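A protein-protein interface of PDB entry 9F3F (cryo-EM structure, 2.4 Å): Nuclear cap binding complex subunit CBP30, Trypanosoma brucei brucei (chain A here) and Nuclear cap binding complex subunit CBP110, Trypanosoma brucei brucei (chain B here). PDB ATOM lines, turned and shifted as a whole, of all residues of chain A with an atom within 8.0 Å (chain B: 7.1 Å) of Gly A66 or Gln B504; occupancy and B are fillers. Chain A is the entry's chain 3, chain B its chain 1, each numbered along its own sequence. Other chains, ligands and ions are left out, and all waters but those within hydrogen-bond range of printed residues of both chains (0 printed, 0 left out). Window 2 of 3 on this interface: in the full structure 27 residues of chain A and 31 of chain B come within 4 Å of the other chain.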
ATOM      1  N   LYS A  63      33.277 -10.217   2.974  1.00  0.00           N
ATOM      2  CA  LYS A  63      32.018  -9.995   2.292  1.00  0.00           C
ATOM      3  C   LYS A  63      32.259  -9.734   0.808  1.00  0.00           C
ATOM      4  O   LYS A  63      33.386  -9.516   0.358  1.00  0.00           O
ATOM      5  CB  LYS A  63      31.269  -8.822   2.921  1.00  0.00           C
ATOM      6  CG  LYS A  63      30.994  -8.982   4.399  1.00  0.00           C
ATOM      7  CD  LYS A  63      30.304  -7.760   4.978  1.00  0.00           C
ATOM      8  CE  LYS A  63      29.109  -7.346   4.146  1.00  0.00           C
ATOM      9  NZ  LYS A  63      28.024  -8.363   4.189  1.00  0.00           N
ATOM     10  N   PHE A  64      31.175  -9.767   0.038  1.00  0.00           N
ATOM     11  CA  PHE A  64      31.270  -9.481  -1.384  1.00  0.00           C
ATOM     12  C   PHE A  64      31.646  -8.024  -1.611  1.00  0.00           C
ATOM     13  O   PHE A  64      31.326  -7.145  -0.807  1.00  0.00           O
ATOM     14  CB  PHE A  64      29.954  -9.802  -2.087  1.00  0.00           C
ATOM     15  CG  PHE A  64      29.990 -11.066  -2.892  1.00  0.00           C
ATOM     16  CD1 PHE A  64      30.759 -11.153  -4.036  1.00  0.00           C
ATOM     17  CD2 PHE A  64      29.252 -12.168  -2.504  1.00  0.00           C
ATOM     18  CE1 PHE A  64      30.789 -12.314  -4.778  1.00  0.00           C
ATOM     19  CE2 PHE A  64      29.275 -13.327  -3.243  1.00  0.00           C
ATOM     20  CZ  PHE A  64      30.046 -13.403  -4.380  1.00  0.00           C
ATOM     21  N   ALA A  65      32.339  -7.777  -2.725  1.00  0.00           N
ATOM     22  CA  ALA A  65      32.800  -6.426  -3.025  1.00  0.00           C
ATOM     23  C   ALA A  65      31.631  -5.462  -3.149  1.00  0.00           C
ATOM     24  O   ALA A  65      31.692  -4.334  -2.647  1.00  0.00           O
ATOM     25  CB  ALA A  65      33.637  -6.430  -4.302  1.00  0.00           C
ATOM     26  N   GLY A  66      30.557  -5.886  -3.814  1.00  0.00           N
ATOM     27  CA  GLY A  66      29.366  -5.057  -3.872  1.00  0.00           C
ATOM     28  C   GLY A  66      28.719  -4.875  -2.514  1.00  0.00           C
ATOM     29  O   GLY A  66      28.218  -3.795  -2.193  1.00  0.00           O
ATOM     30  N   ASP A  67      28.711  -5.933  -1.702  1.00  0.00           N
ATOM     31  CA  ASP A  67      28.161  -5.828  -0.354  1.00  0.00           C
ATOM     32  C   ASP A  67      28.982  -4.873   0.500  1.00  0.00           C
ATOM     33  O   ASP A  67      28.427  -4.086   1.274  1.00  0.00           O
ATOM     34  CB  ASP A  67      28.094  -7.211   0.288  1.00  0.00           C
ATOM     35  CG  ASP A  67      27.278  -8.187  -0.531  1.00  0.00           C
ATOM     36  OD1 ASP A  67      26.742  -7.778  -1.583  1.00  0.00           O
ATOM     37  OD2 ASP A  67      27.174  -9.362  -0.130  1.00  0.00           O
ATOM     38  N   ILE A  68      30.310  -4.934   0.378  1.00  0.00           N
ATOM     39  CA  ILE A  68      31.164  -3.956   1.045  1.00  0.00           C
ATOM     40  C   ILE A  68      30.925  -2.572   0.464  1.00  0.00           C
ATOM     41  O   ILE A  68      30.922  -1.567   1.187  1.00  0.00           O
ATOM     42  CB  ILE A  68      32.641  -4.372   0.931  1.00  0.00           C
ATOM     43  CG1 ILE A  68      32.893  -5.661   1.710  1.00  0.00           C
ATOM     44  CG2 ILE A  68      33.552  -3.269   1.439  1.00  0.00           C
ATOM     45  CD1 ILE A  68      34.338  -6.084   1.733  1.00  0.00           C
ATOM     46  N   GLU A  69      30.689  -2.499  -0.847  1.00  0.00           N
ATOM     47  CA  GLU A  69      30.444  -1.222  -1.504  1.00  0.00           C
ATOM     48  C   GLU A  69      29.159  -0.565  -1.026  1.00  0.00           C
ATOM     49  O   GLU A  69      28.938   0.617  -1.309  1.00  0.00           O
ATOM     50  CB  GLU A  69      30.398  -1.410  -3.020  1.00  0.00           C
ATOM     51  CG  GLU A  69      30.902  -0.217  -3.811  1.00  0.00           C
ATOM     52  CD  GLU A  69      32.339   0.136  -3.483  1.00  0.00           C
ATOM     53  OE1 GLU A  69      33.222  -0.728  -3.667  1.00  0.00           O
ATOM     54  OE2 GLU A  69      32.587   1.278  -3.042  1.00  0.00           O
ATOM     55  N   ALA A  70      28.308  -1.298  -0.312  1.00  0.00           N
ATOM     56  CA  ALA A  70      27.088  -0.732   0.259  1.00  0.00           C
ATOM     57  C   ALA A  70      27.422   0.107   1.495  1.00  0.00           C
ATOM     58  O   ALA A  70      26.988  -0.161   2.615  1.00  0.00           O
ATOM     59  CB  ALA A  70      26.097  -1.840   0.585  1.00  0.00           C
ATOM     60  N   GLU A  71      28.242   1.132   1.264  1.00  0.00           N
ATOM     61  CA  GLU A  71      28.551   2.147   2.260  1.00  0.00           C
ATOM     62  C   GLU A  71      27.611   3.342   2.181  1.00  0.00           C
ATOM     63  O   GLU A  71      27.687   4.230   3.035  1.00  0.00           O
ATOM     64  CB  GLU A  71      29.998   2.620   2.103  1.00  0.00           C
ATOM     65  CG  GLU A  71      31.035   1.556   2.403  1.00  0.00           C
ATOM     66  CD  GLU A  71      32.210   1.597   1.443  1.00  0.00           C
ATOM     67  OE1 GLU A  71      32.144   2.349   0.449  1.00  0.00           O
ATOM     68  OE2 GLU A  71      33.204   0.880   1.685  1.00  0.00           O
ATOM     69  N   GLY A  74      23.144   1.056   1.722  1.00  0.00           N
ATOM     70  CA  GLY A  74      22.509   0.031   0.930  1.00  0.00           C
ATOM     71  C   GLY A  74      22.690  -1.373   1.447  1.00  0.00           C
ATOM     72  O   GLY A  74      22.207  -2.323   0.825  1.00  0.00           O
ATOM     73  N   GLU A  75      23.373  -1.536   2.577  1.00  0.00           N
ATOM     74  CA  GLU A  75      23.646  -2.852   3.128  1.00  0.00           C
ATOM     75  C   GLU A  75      22.422  -3.364   3.881  1.00  0.00           C
ATOM     76  O   GLU A  75      21.387  -2.699   3.960  1.00  0.00           O
ATOM     77  CB  GLU A  75      24.878  -2.799   4.028  1.00  0.00           C
ATOM     78  CG  GLU A  75      25.877  -3.916   3.779  1.00  0.00           C
ATOM     79  CD  GLU A  75      27.200  -3.678   4.480  1.00  0.00           C
ATOM     80  OE1 GLU A  75      27.868  -2.669   4.164  1.00  0.00           O
ATOM     81  OE2 GLU A  75      27.573  -4.499   5.345  1.00  0.00           O
ATOM     82  N   GLY A  76      22.540  -4.563   4.445  1.00  0.00           N
ATOM     83  CA  GLY A  76      21.443  -5.184   5.145  1.00  0.00           C
ATOM     84  C   GLY A  76      21.123  -4.503   6.460  1.00  0.00           C
ATOM     85  O   GLY A  76      21.943  -4.474   7.381  1.00  0.00           O
ATOM     86  N   ARG B 499      14.641 -10.121   2.602  1.00  0.00           N
ATOM     87  CA  ARG B 499      15.157  -9.055   1.751  1.00  0.00           C
ATOM     88  C   ARG B 499      16.016  -8.088   2.553  1.00  0.00           C
ATOM     89  O   ARG B 499      17.106  -7.698   2.120  1.00  0.00           O
ATOM     90  CB  ARG B 499      13.999  -8.310   1.088  1.00  0.00           C
ATOM     91  CG  ARG B 499      13.200  -9.117   0.076  1.00  0.00           C
ATOM     92  CD  ARG B 499      12.101  -8.299  -0.576  1.00  0.00           C
ATOM     93  NE  ARG B 499      11.306  -9.110  -1.488  1.00  0.00           N
ATOM     94  CZ  ARG B 499      10.211  -8.689  -2.107  1.00  0.00           C
ATOM     95  NH1 ARG B 499       9.746  -7.462  -1.932  1.00  0.00           N
ATOM     96  NH2 ARG B 499       9.568  -9.518  -2.923  1.00  0.00           N
ATOM     97  N   ILE B 501      17.510  -8.660   5.519  1.00  0.00           N
ATOM     98  CA  ILE B 501      18.685  -9.309   6.088  1.00  0.00           C
ATOM     99  C   ILE B 501      19.727  -9.582   5.012  1.00  0.00           C
ATOM    100  O   ILE B 501      20.914  -9.284   5.186  1.00  0.00           O
ATOM    101  CB  ILE B 501      18.281 -10.600   6.823  1.00  0.00           C
ATOM    102  CG1 ILE B 501      17.579 -10.273   8.141  1.00  0.00           C
ATOM    103  CG2 ILE B 501      19.494 -11.477   7.073  1.00  0.00           C
ATOM    104  CD1 ILE B 501      18.062  -8.995   8.795  1.00  0.00           C
ATOM    105  N   LEU B 502      19.303 -10.145   3.890  1.00  0.00           N
ATOM    106  CA  LEU B 502      20.257 -10.622   2.901  1.00  0.00           C
ATOM    107  C   LEU B 502      20.914  -9.449   2.181  1.00  0.00           C
ATOM    108  O   LEU B 502      20.255  -8.450   1.880  1.00  0.00           O
ATOM    109  CB  LEU B 502      19.570 -11.535   1.892  1.00  0.00           C
ATOM    110  CG  LEU B 502      19.200 -12.921   2.410  1.00  0.00           C
ATOM    111  CD1 LEU B 502      18.456 -13.700   1.345  1.00  0.00           C
ATOM    112  CD2 LEU B 502      20.442 -13.663   2.849  1.00  0.00           C
ATOM    113  N   PRO B 503      22.208  -9.540   1.890  1.00  0.00           N
ATOM    114  CA  PRO B 503      22.880  -8.451   1.174  1.00  0.00           C
ATOM    115  C   PRO B 503      22.517  -8.417  -0.298  1.00  0.00           C
ATOM    116  O   PRO B 503      21.790  -9.286  -0.789  1.00  0.00           O
ATOM    117  CB  PRO B 503      24.364  -8.768   1.379  1.00  0.00           C
ATOM    118  CG  PRO B 503      24.403 -10.235   1.559  1.00  0.00           C
ATOM    119  CD  PRO B 503      23.141 -10.611   2.270  1.00  0.00           C
ATOM    120  N   GLN B 504      23.027  -7.415  -1.014  1.00  0.00           N
ATOM    121  CA  GLN B 504      22.720  -7.261  -2.429  1.00  0.00           C
ATOM    122  C   GLN B 504      23.293  -8.387  -3.280  1.00  0.00           C
ATOM    123  O   GLN B 504      22.888  -8.530  -4.438  1.00  0.00           O
ATOM    124  CB  GLN B 504      23.204  -5.882  -2.905  1.00  0.00           C
ATOM    125  CG  GLN B 504      24.692  -5.739  -3.239  1.00  0.00           C
ATOM    126  CD  GLN B 504      25.092  -6.369  -4.558  1.00  0.00           C
ATOM    127  OE1 GLN B 504      24.313  -6.393  -5.509  1.00  0.00           O
ATOM    128  NE2 GLN B 504      26.312  -6.888  -4.619  1.00  0.00           N
ATOM    129  N   SER B 505      24.203  -9.192  -2.740  1.00  0.00           N
ATOM    130  CA  SER B 505      24.735 -10.333  -3.469  1.00  0.00           C
ATOM    131  C   SER B 505      23.760 -11.496  -3.547  1.00  0.00           C
ATOM    132  O   SER B 505      24.021 -12.453  -4.281  1.00  0.00           O
ATOM    133  CB  SER B 505      26.034 -10.811  -2.827  1.00  0.00           C
ATOM    134  OG  SER B 505      26.262 -12.174  -3.132  1.00  0.00           O
ATOM    135  N   PHE B 506      22.662 -11.444  -2.799  1.00  0.00           N
ATOM    136  CA  PHE B 506      21.639 -12.476  -2.820  1.00  0.00           C
ATOM    137  C   PHE B 506      20.433 -12.076  -3.652  1.00  0.00           C
ATOM    138  O   PHE B 506      19.388 -12.728  -3.564  1.00  0.00           O
ATOM    139  CB  PHE B 506      21.201 -12.809  -1.394  1.00  0.00           C
ATOM    140  CG  PHE B 506      22.128 -13.742  -0.682  1.00  0.00           C
ATOM    141  CD1 PHE B 506      23.282 -13.272  -0.092  1.00  0.00           C
ATOM    142  CD2 PHE B 506      21.842 -15.088  -0.598  1.00  0.00           C
ATOM    143  CE1 PHE B 506      24.135 -14.126   0.564  1.00  0.00           C
ATOM    144  CE2 PHE B 506      22.692 -15.947   0.057  1.00  0.00           C
ATOM    145  CZ  PHE B 506      23.840 -15.465   0.639  1.00  0.00           C
ATOM    146  N   ASP B 507      20.549 -11.012  -4.450  1.00  0.00           N
ATOM    147  CA  ASP B 507      19.424 -10.567  -5.262  1.00  0.00           C
ATOM    148  C   ASP B 507      19.018 -11.627  -6.274  1.00  0.00           C
ATOM    149  O   ASP B 507      17.824 -11.850  -6.499  1.00  0.00           O
ATOM    150  CB  ASP B 507      19.771  -9.255  -5.961  1.00  0.00           C
ATOM    151  CG  ASP B 507      19.740  -8.072  -5.020  1.00  0.00           C
ATOM    152  OD1 ASP B 507      19.973  -8.271  -3.810  1.00  0.00           O
ATOM    153  OD2 ASP B 507      19.475  -6.945  -5.486  1.00  0.00           O
ATOM    154  N   VAL B 508      19.990 -12.293  -6.897  1.00  0.00           N
ATOM    155  CA  VAL B 508      19.665 -13.378  -7.818  1.00  0.00           C
ATOM    156  C   VAL B 508      18.977 -14.514  -7.070  1.00  0.00           C
ATOM    157  O   VAL B 508      17.950 -15.045  -7.512  1.00  0.00           O
ATOM    158  CB  VAL B 508      20.929 -13.862  -8.549  1.00  0.00           C
ATOM    159  CG1 VAL B 508      20.626 -15.100  -9.364  1.00  0.00           C
ATOM    160  CG2 VAL B 508      21.473 -12.764  -9.437  1.00  0.00           C
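The side-chain amide nitrogen (NE2) of Gln B504 is in hydrogen-bond range of the side-chain carboxylate (OD1) of Asp A67 (3.2 Å).
N of Ser B505 sits at hydrogen-bond distance from OD1 of Asp A67 (3.1 Å).
CD2 of Phe A64 touches OG of Ser B505, at 3.1 Å.
Gly A66 touches Gln B504 (CA to NE2, 3.6 Å).
Pro B503 touches Asp A67.
Of chain B, only Gln B504 (3.6 Å) comes within 4 Å of Gly A66.
Gln B504 touches just these residues of chain A: Gly A66 and Asp A67.
Of the printed residues of chain B, Phe A64 touches Ser B505 (3.1 Å).
Of the printed residues of chain B, Asp A67 touches Pro B503 (3.2 Å), Gln B504 (3.2 Å) and Ser B505 (3.1 Å).
Ala A70 touches none of the printed residues of chain B.
The nearest residue of chain B that does not touch Gly A66 is Ser B505 (6.3 Å).
The nearest residue of chain A that does not touch Gln B504 is Gly A74 (5.3 Å).
Hydrophobic or aromatic side chains of chain A that line the printed part of chain B: Phe A64.
Hydrophobic or aromatic side chains of chain B within 4 Å of the printed part of chain A: Pro B503.
Among the printed residues, 5 pairs touch across the chains.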
